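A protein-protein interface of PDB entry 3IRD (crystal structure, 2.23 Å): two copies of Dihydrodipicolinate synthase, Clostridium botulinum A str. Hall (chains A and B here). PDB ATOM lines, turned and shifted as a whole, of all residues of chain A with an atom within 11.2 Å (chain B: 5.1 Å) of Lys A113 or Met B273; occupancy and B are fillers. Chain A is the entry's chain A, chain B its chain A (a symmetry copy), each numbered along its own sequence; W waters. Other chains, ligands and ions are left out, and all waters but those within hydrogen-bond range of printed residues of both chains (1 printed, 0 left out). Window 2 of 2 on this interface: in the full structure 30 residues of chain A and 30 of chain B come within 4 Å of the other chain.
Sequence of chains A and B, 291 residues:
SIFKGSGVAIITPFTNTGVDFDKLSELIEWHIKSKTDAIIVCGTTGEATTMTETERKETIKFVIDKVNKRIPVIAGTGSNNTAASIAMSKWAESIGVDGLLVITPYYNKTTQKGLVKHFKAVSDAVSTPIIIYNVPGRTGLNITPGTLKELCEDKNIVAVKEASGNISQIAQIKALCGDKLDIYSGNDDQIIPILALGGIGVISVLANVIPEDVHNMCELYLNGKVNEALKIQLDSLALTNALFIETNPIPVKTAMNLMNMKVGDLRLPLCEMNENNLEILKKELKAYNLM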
ATOM      1  N   THR A  82      35.308  -5.001 -19.879  1.00  0.00           N
ATOM      2  CA  THR A  82      35.607  -5.931 -18.783  1.00  0.00           C
ATOM      3  C   THR A  82      36.725  -5.406 -17.821  1.00  0.00           C
ATOM      4  O   THR A  82      36.586  -5.522 -16.606  1.00  0.00           O
ATOM      5  CB  THR A  82      35.974  -7.332 -19.325  1.00  0.00           C
ATOM      6  OG1 THR A  82      34.927  -7.855 -20.150  1.00  0.00           O
ATOM      7  CG2 THR A  82      36.252  -8.296 -18.217  1.00  0.00           C
ATOM      8  N   THR A 104      25.282  -6.974 -17.645  1.00  0.00           N
ATOM      9  CA  THR A 104      25.845  -7.585 -18.851  1.00  0.00           C
ATOM     10  C   THR A 104      26.480  -6.438 -19.682  1.00  0.00           C
ATOM     11  O   THR A 104      26.157  -5.283 -19.482  1.00  0.00           O
ATOM     12  CB  THR A 104      24.765  -8.238 -19.738  1.00  0.00           C
ATOM     13  OG1 THR A 104      23.871  -7.237 -20.215  1.00  0.00           O
ATOM     14  CG2 THR A 104      23.987  -9.386 -19.008  1.00  0.00           C
ATOM     15  N   PRO A 105      27.426  -6.762 -20.587  1.00  0.00           N
ATOM     16  CA  PRO A 105      27.857  -5.740 -21.531  1.00  0.00           C
ATOM     17  C   PRO A 105      26.647  -5.240 -22.352  1.00  0.00           C
ATOM     18  O   PRO A 105      25.629  -5.925 -22.452  1.00  0.00           O
ATOM     19  CB  PRO A 105      28.850  -6.467 -22.435  1.00  0.00           C
ATOM     20  CG  PRO A 105      29.310  -7.610 -21.668  1.00  0.00           C
ATOM     21  CD  PRO A 105      28.205  -8.011 -20.710  1.00  0.00           C
ATOM     22  N   LYS A 109      28.138  -5.376 -26.706  1.00  0.00           N
ATOM     23  CA  LYS A 109      27.555  -6.707 -26.536  1.00  0.00           C
ATOM     24  C   LYS A 109      28.636  -7.792 -26.604  1.00  0.00           C
ATOM     25  O   LYS A 109      29.818  -7.454 -26.463  1.00  0.00           O
ATOM     26  CB  LYS A 109      26.431  -6.917 -27.546  1.00  0.00           C
ATOM     27  CG  LYS A 109      25.398  -5.782 -27.415  1.00  0.00           C
ATOM     28  CD  LYS A 109      24.070  -6.185 -27.965  1.00  0.00           C
ATOM     29  CE  LYS A 109      24.139  -6.464 -29.439  1.00  0.00           C
ATOM     30  NZ  LYS A 109      22.961  -7.334 -29.822  1.00  0.00           N
ATOM     31  N   THR A 110      28.219  -9.065 -26.756  1.00  0.00           N
ATOM     32  CA  THR A 110      29.102 -10.223 -26.944  1.00  0.00           C
ATOM     33  C   THR A 110      28.220 -11.494 -27.061  1.00  0.00           C
ATOM     34  O   THR A 110      26.994 -11.380 -27.086  1.00  0.00           O
ATOM     35  CB  THR A 110      30.145 -10.359 -25.797  1.00  0.00           C
ATOM     36  OG1 THR A 110      31.087 -11.395 -26.106  1.00  0.00           O
ATOM     37  CG2 THR A 110      29.496 -10.653 -24.427  1.00  0.00           C
ATOM     38  N   THR A 111      28.824 -12.685 -27.144  1.00  0.00           N
ATOM     39  CA  THR A 111      28.073 -13.930 -27.270  1.00  0.00           C
ATOM     40  C   THR A 111      27.783 -14.484 -25.890  1.00  0.00           C
ATOM     41  O   THR A 111      28.301 -13.999 -24.881  1.00  0.00           O
ATOM     42  CB  THR A 111      28.877 -15.000 -28.052  1.00  0.00           C
ATOM     43  OG1 THR A 111      30.190 -15.144 -27.480  1.00  0.00           O
ATOM     44  CG2 THR A 111      29.003 -14.601 -29.538  1.00  0.00           C
ATOM     45  N   GLN A 112      27.034 -15.556 -25.832  1.00  0.00           N
ATOM     46  CA  GLN A 112      26.855 -16.231 -24.563  1.00  0.00           C
ATOM     47  C   GLN A 112      28.219 -16.724 -24.008  1.00  0.00           C
ATOM     48  O   GLN A 112      28.467 -16.718 -22.765  1.00  0.00           O
ATOM     49  CB  GLN A 112      25.827 -17.393 -24.735  1.00  0.00           C
ATOM     50  CG  GLN A 112      24.398 -16.935 -25.130  1.00  0.00           C
ATOM     51  CD  GLN A 112      23.788 -15.896 -24.124  1.00  0.00           C
ATOM     52  OE1 GLN A 112      23.760 -16.096 -22.902  1.00  0.00           O
ATOM     53  NE2 GLN A 112      23.281 -14.791 -24.668  1.00  0.00           N
ATOM     54  N   LYS A 113      29.084 -17.191 -24.921  1.00  0.00           N
ATOM     55  CA  LYS A 113      30.434 -17.621 -24.593  1.00  0.00           C
ATOM     56  C   LYS A 113      31.211 -16.471 -23.961  1.00  0.00           C
ATOM     57  O   LYS A 113      31.838 -16.662 -22.926  1.00  0.00           O
ATOM     58  CB  LYS A 113      31.136 -18.162 -25.826  1.00  0.00           C
ATOM     59  CG  LYS A 113      32.505 -18.760 -25.520  1.00  0.00           C
ATOM     60  CD  LYS A 113      33.154 -19.182 -26.789  1.00  0.00           C
ATOM     61  CE  LYS A 113      34.550 -19.616 -26.504  1.00  0.00           C
ATOM     62  NZ  LYS A 113      35.134 -19.859 -27.822  1.00  0.00           N
ATOM     63  N   GLY A 114      31.146 -15.263 -24.548  1.00  0.00           N
ATOM     64  CA  GLY A 114      31.796 -14.079 -23.932  1.00  0.00           C
ATOM     65  C   GLY A 114      31.223 -13.601 -22.577  1.00  0.00           C
ATOM     66  O   GLY A 114      31.943 -13.102 -21.725  1.00  0.00           O
ATOM     67  N   LEU A 115      29.911 -13.736 -22.399  1.00  0.00           N
ATOM     68  CA  LEU A 115      29.253 -13.423 -21.134  1.00  0.00           C
ATOM     69  C   LEU A 115      29.854 -14.255 -20.001  1.00  0.00           C
ATOM     70  O   LEU A 115      30.197 -13.724 -18.951  1.00  0.00           O
ATOM     71  CB  LEU A 115      27.739 -13.700 -21.258  1.00  0.00           C
ATOM     72  CG  LEU A 115      26.918 -12.638 -22.015  1.00  0.00           C
ATOM     73  CD1 LEU A 115      25.508 -13.200 -22.269  1.00  0.00           C
ATOM     74  CD2 LEU A 115      26.833 -11.250 -21.219  1.00  0.00           C
ATOM     75  N   VAL A 116      30.001 -15.554 -20.228  1.00  0.00           N
ATOM     76  CA  VAL A 116      30.675 -16.418 -19.255  1.00  0.00           C
ATOM     77  C   VAL A 116      32.089 -15.896 -18.959  1.00  0.00           C
ATOM     78  O   VAL A 116      32.428 -15.701 -17.792  1.00  0.00           O
ATOM     79  CB  VAL A 116      30.735 -17.886 -19.715  1.00  0.00           C
ATOM     80  CG1 VAL A 116      31.630 -18.720 -18.776  1.00  0.00           C
ATOM     81  CG2 VAL A 116      29.304 -18.469 -19.751  1.00  0.00           C
ATOM     82  N   LYS A 117      32.900 -15.642 -19.986  1.00  0.00           N
ATOM     83  CA  LYS A 117      34.253 -15.136 -19.703  1.00  0.00           C
ATOM     84  C   LYS A 117      34.228 -13.749 -19.027  1.00  0.00           C
ATOM     85  O   LYS A 117      35.021 -13.486 -18.119  1.00  0.00           O
ATOM     86  CB  LYS A 117      35.105 -15.091 -20.967  1.00  0.00           C
ATOM     87  CG  LYS A 117      35.243 -16.459 -21.661  1.00  0.00           C
ATOM     88  CD  LYS A 117      35.978 -16.319 -23.012  1.00  0.00           C
ATOM     89  CE  LYS A 117      36.315 -17.696 -23.622  1.00  0.00           C
ATOM     90  NZ  LYS A 117      37.483 -18.277 -22.926  1.00  0.00           N
ATOM     91  N   HIS A 118      33.335 -12.862 -19.492  1.00  0.00           N
ATOM     92  CA  HIS A 118      33.143 -11.558 -18.863  1.00  0.00           C
ATOM     93  C   HIS A 118      32.902 -11.651 -17.348  1.00  0.00           C
ATOM     94  O   HIS A 118      33.637 -11.094 -16.544  1.00  0.00           O
ATOM     95  CB  HIS A 118      32.005 -10.776 -19.521  1.00  0.00           C
ATOM     96  CG  HIS A 118      31.707  -9.487 -18.825  1.00  0.00           C
ATOM     97  ND1 HIS A 118      32.540  -8.377 -18.919  1.00  0.00           N
ATOM     98  CD2 HIS A 118      30.661  -9.120 -18.033  1.00  0.00           C
ATOM     99  CE1 HIS A 118      32.018  -7.391 -18.208  1.00  0.00           C
ATOM    100  NE2 HIS A 118      30.879  -7.810 -17.664  1.00  0.00           N
ATOM    101  N   PHE A 119      31.881 -12.402 -16.974  1.00  0.00           N
ATOM    102  CA  PHE A 119      31.505 -12.473 -15.576  1.00  0.00           C
ATOM    103  C   PHE A 119      32.485 -13.260 -14.738  1.00  0.00           C
ATOM    104  O   PHE A 119      32.642 -12.962 -13.574  1.00  0.00           O
ATOM    105  CB  PHE A 119      30.092 -13.033 -15.444  1.00  0.00           C
ATOM    106  CG  PHE A 119      29.034 -12.011 -15.747  1.00  0.00           C
ATOM    107  CD1 PHE A 119      28.340 -12.033 -16.952  1.00  0.00           C
ATOM    108  CD2 PHE A 119      28.745 -11.012 -14.824  1.00  0.00           C
ATOM    109  CE1 PHE A 119      27.370 -11.077 -17.223  1.00  0.00           C
ATOM    110  CE2 PHE A 119      27.790 -10.037 -15.066  1.00  0.00           C
ATOM    111  CZ  PHE A 119      27.102 -10.066 -16.259  1.00  0.00           C
ATOM    112  N   LYS A 120      33.158 -14.250 -15.331  1.00  0.00           N
ATOM    113  CA  LYS A 120      34.185 -15.009 -14.609  1.00  0.00           C
ATOM    114  C   LYS A 120      35.383 -14.105 -14.377  1.00  0.00           C
ATOM    115  O   LYS A 120      36.045 -14.242 -13.328  1.00  0.00           O
ATOM    116  CB  LYS A 120      34.627 -16.315 -15.326  1.00  0.00           C
ATOM    117  CG  LYS A 120      33.600 -17.491 -15.269  1.00  0.00           C
ATOM    118  CD  LYS A 120      33.311 -18.041 -13.820  1.00  0.00           C
ATOM    119  CE  LYS A 120      34.601 -18.350 -13.044  1.00  0.00           C
ATOM    120  NZ  LYS A 120      34.368 -19.012 -11.713  1.00  0.00           N
ATOM    121  N   ALA A 121      35.669 -13.173 -15.310  1.00  0.00           N
ATOM    122  CA  ALA A 121      36.876 -12.381 -15.123  1.00  0.00           C
ATOM    123  C   ALA A 121      36.647 -11.351 -14.000  1.00  0.00           C
ATOM    124  O   ALA A 121      37.564 -11.085 -13.192  1.00  0.00           O
ATOM    125  CB  ALA A 121      37.341 -11.710 -16.439  1.00  0.00           C
ATOM    126  N   LEU A 141      21.047  -7.021 -25.244  1.00  0.00           N
ATOM    127  CA  LEU A 141      21.665  -8.327 -25.019  1.00  0.00           C
ATOM    128  C   LEU A 141      20.932  -9.020 -23.900  1.00  0.00           C
ATOM    129  O   LEU A 141      20.709  -8.392 -22.875  1.00  0.00           O
ATOM    130  CB  LEU A 141      23.164  -8.179 -24.686  1.00  0.00           C
ATOM    131  CG  LEU A 141      24.022  -9.416 -24.382  1.00  0.00           C
ATOM    132  CD1 LEU A 141      23.902 -10.505 -25.474  1.00  0.00           C
ATOM    133  CD2 LEU A 141      25.485  -9.065 -24.114  1.00  0.00           C
ATOM    134  N   ASN A 142      20.599 -10.306 -24.133  1.00  0.00           N
ATOM    135  CA  ASN A 142      19.886 -11.184 -23.211  1.00  0.00           C
ATOM    136  C   ASN A 142      20.759 -12.347 -22.715  1.00  0.00           C
ATOM    137  O   ASN A 142      21.246 -13.157 -23.495  1.00  0.00           O
ATOM    138  CB  ASN A 142      18.546 -11.705 -23.833  1.00  0.00           C
ATOM    139  CG  ASN A 142      17.707 -12.495 -22.819  1.00  0.00           C
ATOM    140  OD1 ASN A 142      17.443 -12.036 -21.666  1.00  0.00           O
ATOM    141  ND2 ASN A 142      17.291 -13.726 -23.228  1.00  0.00           N
ATOM    142  N   ILE A 143      21.010 -12.388 -21.401  1.00  0.00           N
ATOM    143  CA  ILE A 143      21.746 -13.501 -20.869  1.00  0.00           C
ATOM    144  C   ILE A 143      20.718 -14.573 -20.636  1.00  0.00           C
ATOM    145  O   ILE A 143      19.693 -14.335 -20.022  1.00  0.00           O
ATOM    146  CB  ILE A 143      22.602 -13.113 -19.666  1.00  0.00           C
ATOM    147  CG1 ILE A 143      23.488 -14.285 -19.259  1.00  0.00           C
ATOM    148  CG2 ILE A 143      21.751 -12.615 -18.536  1.00  0.00           C
ATOM    149  CD1 ILE A 143      24.742 -13.952 -18.303  1.00  0.00           C
ATOM    150  N   THR A 144      20.951 -15.749 -21.197  1.00  0.00           N
ATOM    151  CA  THR A 144      19.906 -16.787 -21.191  1.00  0.00           C
ATOM    152  C   THR A 144      19.891 -17.556 -19.890  1.00  0.00           C
ATOM    153  O   THR A 144      20.825 -17.470 -19.124  1.00  0.00           O
ATOM    154  CB  THR A 144      20.109 -17.814 -22.349  1.00  0.00           C
ATOM    155  OG1 THR A 144      21.322 -18.514 -22.109  1.00  0.00           O
ATOM    156  CG2 THR A 144      20.162 -17.114 -23.738  1.00  0.00           C
ATOM    157  N   GLY A 146      20.375 -20.796 -19.648  1.00  0.00           N
ATOM    158  CA  GLY A 146      21.517 -21.724 -19.731  1.00  0.00           C
ATOM    159  C   GLY A 146      22.850 -21.050 -19.350  1.00  0.00           C
ATOM    160  O   GLY A 146      23.728 -21.658 -18.739  1.00  0.00           O
ATOM    161  N   THR A 147      23.040 -19.795 -19.763  1.00  0.00           N
ATOM    162  CA  THR A 147      24.313 -19.134 -19.431  1.00  0.00           C
ATOM    163  C   THR A 147      24.309 -18.870 -17.932  1.00  0.00           C
ATOM    164  O   THR A 147      25.330 -19.036 -17.272  1.00  0.00           O
ATOM    165  CB  THR A 147      24.497 -17.844 -20.194  1.00  0.00           C
ATOM    166  OG1 THR A 147      24.548 -18.139 -21.596  1.00  0.00           O
ATOM    167  CG2 THR A 147      25.778 -17.130 -19.743  1.00  0.00           C
ATOM    168  N   LEU A 148      23.145 -18.514 -17.389  1.00  0.00           N
ATOM    169  CA  LEU A 148      23.073 -18.240 -15.962  1.00  0.00           C
ATOM    170  C   LEU A 148      23.356 -19.521 -15.132  1.00  0.00           C
ATOM    171  O   LEU A 148      24.113 -19.461 -14.155  1.00  0.00           O
ATOM    172  CB  LEU A 148      21.745 -17.552 -15.568  1.00  0.00           C
ATOM    173  CG  LEU A 148      21.483 -16.056 -15.812  1.00  0.00           C
ATOM    174  CD1 LEU A 148      19.986 -15.640 -15.643  1.00  0.00           C
ATOM    175  CD2 LEU A 148      22.379 -15.191 -14.877  1.00  0.00           C
ATOM    176  N   GLU A 150      25.229 -22.043 -16.020  1.00  0.00           N
ATOM    177  CA  GLU A 150      26.673 -22.215 -15.975  1.00  0.00           C
ATOM    178  C   GLU A 150      27.393 -21.229 -14.976  1.00  0.00           C
ATOM    179  O   GLU A 150      28.322 -21.613 -14.274  1.00  0.00           O
ATOM    180  CB  GLU A 150      27.229 -22.113 -17.408  1.00  0.00           C
ATOM    181  CG  GLU A 150      28.735 -22.266 -17.491  1.00  0.00           C
ATOM    182  CD  GLU A 150      29.245 -22.271 -18.917  1.00  0.00           C
ATOM    183  OE1 GLU A 150      28.433 -22.330 -19.860  1.00  0.00           O
ATOM    184  OE2 GLU A 150      30.470 -22.198 -19.091  1.00  0.00           O
ATOM    185  N   LEU A 151      26.949 -19.983 -14.887  1.00  0.00           N
ATOM    186  CA  LEU A 151      27.619 -19.002 -14.037  1.00  0.00           C
ATOM    187  C   LEU A 151      27.286 -19.205 -12.543  1.00  0.00           C
ATOM    188  O   LEU A 151      28.121 -18.916 -11.661  1.00  0.00           O
ATOM    189  CB  LEU A 151      27.334 -17.575 -14.486  1.00  0.00           C
ATOM    190  CG  LEU A 151      28.128 -17.194 -15.732  1.00  0.00           C
ATOM    191  CD1 LEU A 151      27.593 -15.935 -16.378  1.00  0.00           C
ATOM    192  CD2 LEU A 151      29.630 -17.017 -15.412  1.00  0.00           C
ATOM    193  N   ILE B 245      27.482 -13.758 -37.860  1.00  0.00           N
ATOM    194  CA  ILE B 245      27.085 -14.968 -37.143  1.00  0.00           C
ATOM    195  C   ILE B 245      27.309 -14.887 -35.639  1.00  0.00           C
ATOM    196  O   ILE B 245      26.581 -15.513 -34.882  1.00  0.00           O
ATOM    197  CB  ILE B 245      27.711 -16.234 -37.745  1.00  0.00           C
ATOM    198  CG1 ILE B 245      26.782 -17.444 -37.490  1.00  0.00           C
ATOM    199  CG2 ILE B 245      29.173 -16.397 -37.305  1.00  0.00           C
ATOM    200  CD1 ILE B 245      27.338 -18.776 -38.063  1.00  0.00           C
ATOM    201  N   GLU B 246      28.291 -14.093 -35.219  1.00  0.00           N
ATOM    202  CA  GLU B 246      28.458 -13.712 -33.804  1.00  0.00           C
ATOM    203  C   GLU B 246      28.665 -12.182 -33.770  1.00  0.00           C
ATOM    204  O   GLU B 246      29.015 -11.568 -34.814  1.00  0.00           O
ATOM    205  CB  GLU B 246      29.651 -14.451 -33.169  1.00  0.00           C
ATOM    206  CG  GLU B 246      29.366 -15.903 -32.911  1.00  0.00           C
ATOM    207  CD  GLU B 246      30.497 -16.674 -32.237  1.00  0.00           C
ATOM    208  OE1 GLU B 246      31.422 -16.054 -31.666  1.00  0.00           O
ATOM    209  OE2 GLU B 246      30.428 -17.915 -32.264  1.00  0.00           O
ATOM    210  N   ILE B 250      33.818  -9.787 -33.687  1.00  0.00           N
ATOM    211  CA  ILE B 250      34.354 -11.138 -33.506  1.00  0.00           C
ATOM    212  C   ILE B 250      34.589 -11.847 -34.858  1.00  0.00           C
ATOM    213  O   ILE B 250      35.689 -12.349 -35.084  1.00  0.00           O
ATOM    214  CB  ILE B 250      33.416 -11.989 -32.579  1.00  0.00           C
ATOM    215  CG1 ILE B 250      33.544 -11.520 -31.127  1.00  0.00           C
ATOM    216  CG2 ILE B 250      33.674 -13.465 -32.695  1.00  0.00           C
ATOM    217  CD1 ILE B 250      32.451 -12.083 -30.251  1.00  0.00           C
ATOM    218  N   PRO B 251      33.549 -11.901 -35.754  1.00  0.00           N
ATOM    219  CA  PRO B 251      33.834 -12.665 -36.950  1.00  0.00           C
ATOM    220  C   PRO B 251      34.817 -11.970 -37.910  1.00  0.00           C
ATOM    221  O   PRO B 251      35.624 -12.665 -38.534  1.00  0.00           O
ATOM    222  CB  PRO B 251      32.433 -12.869 -37.595  1.00  0.00           C
ATOM    223  CG  PRO B 251      31.473 -12.778 -36.505  1.00  0.00           C
ATOM    224  CD  PRO B 251      32.107 -11.584 -35.676  1.00  0.00           C
ATOM    225  N   THR B 254      38.325 -12.433 -36.747  1.00  0.00           N
ATOM    226  CA  THR B 254      38.639 -13.858 -36.920  1.00  0.00           C
ATOM    227  C   THR B 254      39.016 -14.131 -38.388  1.00  0.00           C
ATOM    228  O   THR B 254      39.950 -14.863 -38.681  1.00  0.00           O
ATOM    229  CB  THR B 254      37.478 -14.776 -36.493  1.00  0.00           C
ATOM    230  OG1 THR B 254      37.141 -14.511 -35.120  1.00  0.00           O
ATOM    231  CG2 THR B 254      37.882 -16.249 -36.642  1.00  0.00           C
ATOM    232  N   CYS B 271      35.261 -12.303 -27.512  1.00  0.00           N
ATOM    233  CA  CYS B 271      36.138 -13.491 -27.414  1.00  0.00           C
ATOM    234  C   CYS B 271      36.010 -14.357 -28.678  1.00  0.00           C
ATOM    235  O   CYS B 271      35.142 -14.083 -29.572  1.00  0.00           O
ATOM    236  CB  CYS B 271      35.825 -14.336 -26.183  1.00  0.00           C
ATOM    237  SG  CYS B 271      34.242 -15.225 -26.317  1.00  0.00           S
ATOM    238  N   GLU B 272      36.885 -15.359 -28.762  1.00  0.00           N
ATOM    239  CA  GLU B 272      36.946 -16.314 -29.885  1.00  0.00           C
ATOM    240  C   GLU B 272      35.592 -16.953 -30.192  1.00  0.00           C
ATOM    241  O   GLU B 272      34.719 -17.094 -29.312  1.00  0.00           O
ATOM    242  CB  GLU B 272      38.042 -17.386 -29.647  1.00  0.00           C
ATOM    243  CG  GLU B 272      38.223 -17.737 -28.129  1.00  0.00           C
ATOM    244  CD  GLU B 272      38.742 -19.161 -27.856  1.00  0.00           C
ATOM    245  OE1 GLU B 272      39.692 -19.587 -28.577  1.00  0.00           O
ATOM    246  OE2 GLU B 272      38.200 -19.828 -26.898  1.00  0.00           O
ATOM    247  N   MET B 273      35.387 -17.223 -31.478  1.00  0.00           N
ATOM    248  CA  MET B 273      34.137 -17.761 -31.986  1.00  0.00           C
ATOM    249  C   MET B 273      33.927 -19.148 -31.444  1.00  0.00           C
ATOM    250  O   MET B 273      34.893 -19.829 -31.129  1.00  0.00           O
ATOM    251  CB  MET B 273      34.208 -17.863 -33.515  1.00  0.00           C
ATOM    252  CG  MET B 273      34.278 -16.493 -34.166  1.00  0.00           C
ATOM    253  SD  MET B 273      34.115 -16.534 -35.912  1.00  0.00           S
ATOM    254  CE  MET B 273      32.432 -17.060 -36.127  1.00  0.00           C
ATOM    255  N   ASN B 274      32.684 -19.602 -31.355  1.00  0.00           N
ATOM    256  CA  ASN B 274      32.554 -21.039 -31.145  1.00  0.00           C
ATOM    257  C   ASN B 274      32.797 -21.840 -32.448  1.00  0.00           C
ATOM    258  O   ASN B 274      32.840 -21.273 -33.548  1.00  0.00           O
ATOM    259  CB  ASN B 274      31.332 -21.435 -30.299  1.00  0.00           C
ATOM    260  CG  ASN B 274      30.075 -21.466 -31.083  1.00  0.00           C
ATOM    261  OD1 ASN B 274      30.071 -21.727 -32.290  1.00  0.00           O
ATOM    262  ND2 ASN B 274      28.976 -21.211 -30.406  1.00  0.00           N
ATOM    263  N   GLU B 275      33.026 -23.139 -32.285  1.00  0.00           N
ATOM    264  CA  GLU B 275      33.526 -24.013 -33.338  1.00  0.00           C
ATOM    265  C   GLU B 275      32.560 -24.145 -34.536  1.00  0.00           C
ATOM    266  O   GLU B 275      32.961 -23.927 -35.679  1.00  0.00           O
ATOM    267  CB  GLU B 275      33.960 -25.361 -32.711  1.00  0.00           C
ATOM    268  CG  GLU B 275      34.641 -26.434 -33.655  1.00  0.00           C
ATOM    269  CD  GLU B 275      35.728 -25.873 -34.649  1.00  0.00           C
ATOM    270  OE1 GLU B 275      36.736 -25.246 -34.198  1.00  0.00           O
ATOM    271  OE2 GLU B 275      35.570 -26.095 -35.888  1.00  0.00           O
ATOM    272  N   ASN B 277      30.299 -22.126 -35.605  1.00  0.00           N
ATOM    273  CA  ASN B 277      30.200 -20.837 -36.315  1.00  0.00           C
ATOM    274  C   ASN B 277      31.515 -20.534 -37.026  1.00  0.00           C
ATOM    275  O   ASN B 277      31.495 -20.072 -38.128  1.00  0.00           O
ATOM    276  CB  ASN B 277      29.866 -19.695 -35.365  1.00  0.00           C
ATOM    277  CG  ASN B 277      28.547 -19.865 -34.721  1.00  0.00           C
ATOM    278  OD1 ASN B 277      27.687 -20.594 -35.219  1.00  0.00           O
ATOM    279  ND2 ASN B 277      28.374 -19.208 -33.573  1.00  0.00           N
ATOM    280  N   LEU B 278      32.642 -20.849 -36.379  1.00  0.00           N
ATOM    281  CA  LEU B 278      33.958 -20.758 -37.026  1.00  0.00           C
ATOM    282  C   LEU B 278      33.972 -21.529 -38.370  1.00  0.00           C
ATOM    283  O   LEU B 278      34.400 -20.989 -39.397  1.00  0.00           O
ATOM    284  CB  LEU B 278      35.073 -21.223 -36.047  1.00  0.00           C
ATOM    285  CG  LEU B 278      36.506 -21.222 -36.584  1.00  0.00           C
ATOM    286  CD1 LEU B 278      36.939 -19.802 -36.948  1.00  0.00           C
ATOM    287  CD2 LEU B 278      37.542 -21.889 -35.607  1.00  0.00           C
ATOM    288  N   LEU B 281      31.979 -19.749 -41.008  1.00  0.00           N
ATOM    289  CA  LEU B 281      32.765 -18.624 -41.515  1.00  0.00           C
ATOM    290  C   LEU B 281      33.816 -19.065 -42.595  1.00  0.00           C
ATOM    291  O   LEU B 281      33.843 -18.522 -43.731  1.00  0.00           O
ATOM    292  CB  LEU B 281      33.366 -17.806 -40.338  1.00  0.00           C
ATOM    293  CG  LEU B 281      34.273 -16.628 -40.736  1.00  0.00           C
ATOM    294  CD1 LEU B 281      33.523 -15.545 -41.510  1.00  0.00           C
ATOM    295  CD2 LEU B 281      35.026 -16.040 -39.534  1.00  0.00           C
HETATM  296  O   HOH W   1      32.006 -16.233 -29.040  1.00  0.00           O
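The side-chain carboxylate of Glu B272 lies within salt-bridge range of the side-chain amino group of Lys A113, 3.2 Å away. The side-chain amino group (NZ) of Lys A113 lies within hydrogen-bond range of the backbone carbonyl oxygen (O) of Met B273, 3.3 Å away. N of Gly A114 lies within hydrogen-bond range of SG of Cys B271 (3.6 Å).
The side-chain hydroxyl (OG1) of Thr A111 sits close to the backbone NH (N) of Lys A113 (3.5 Å). The side-chain hydroxyl (OG1) of Thr A111 sits at hydrogen-bond distance from the backbone NH (N) of Gly A114. N of Asn B274 is in hydrogen-bond range of OE2 of Glu B246. OE2 of Glu B246 lies within hydrogen-bond range of ND2 of Asn B277 (2.8 Å). The side-chain hydroxyl (OG1) of Thr B254 lies close to the side-chain sulfur (SD) of Met B273 (3.7 Å).
Among the printed residues, merely in contact across the chains: Thr A111 with Glu B246 and Lys A117 with Cys B271.
Printed residues of chain B within 4 Å of Thr A111: Glu B246. Of the printed residues of chain B, Lys A113 touches Glu B272 and Met B273. Printed residues of chain B within 4 Å of Gly A114: Cys B271 (3.6 Å). Printed residues of chain B within 4 Å of Lys A117: Cys B271. Leu A141 touches none of the printed residues of chain B. Leu A151 touches none of the printed residues of chain B. No residue of chain A comes within 4 Å of Ile B245. No residue of chain A comes within 4 Å of Ile B250. Printed residues of chain A within 4 Å of Cys B271: Gly A114 (3.6 Å) and Lys A117 (3.7 Å). Glu B272 touches just one residue of chain A: Lys A113. Of the printed residues of chain A, Met B273 touches Lys A113. No residue of chain A comes within 4 Å of Asn B277. No residue of chain A comes within 4 Å of Leu B278. The nearest printed residue of chain A that does not touch Cys B271 is Lys A113 (4.02 Å).
Among the printed residues, 5 pairs touch across the chains. Among the printed residues, Asp or Glu carboxylates within 4 Å of a Lys or Arg side-chain nitrogen of the other chain: Lys A113 with Glu B272 (3.2 Å).
No position is printed for both chains. Of the 5 pairs that touch across the chains among the printed residues, none has its exchanged pair printed and touching as well.
Water W1 lies within hydrogen-bond range of OG1 of Thr A111 (2.6 Å), OE1 of Glu B246 (2.7 Å), O of Glu B272 (2.9 Å) and SG of Cys B271 (3.7 Å).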
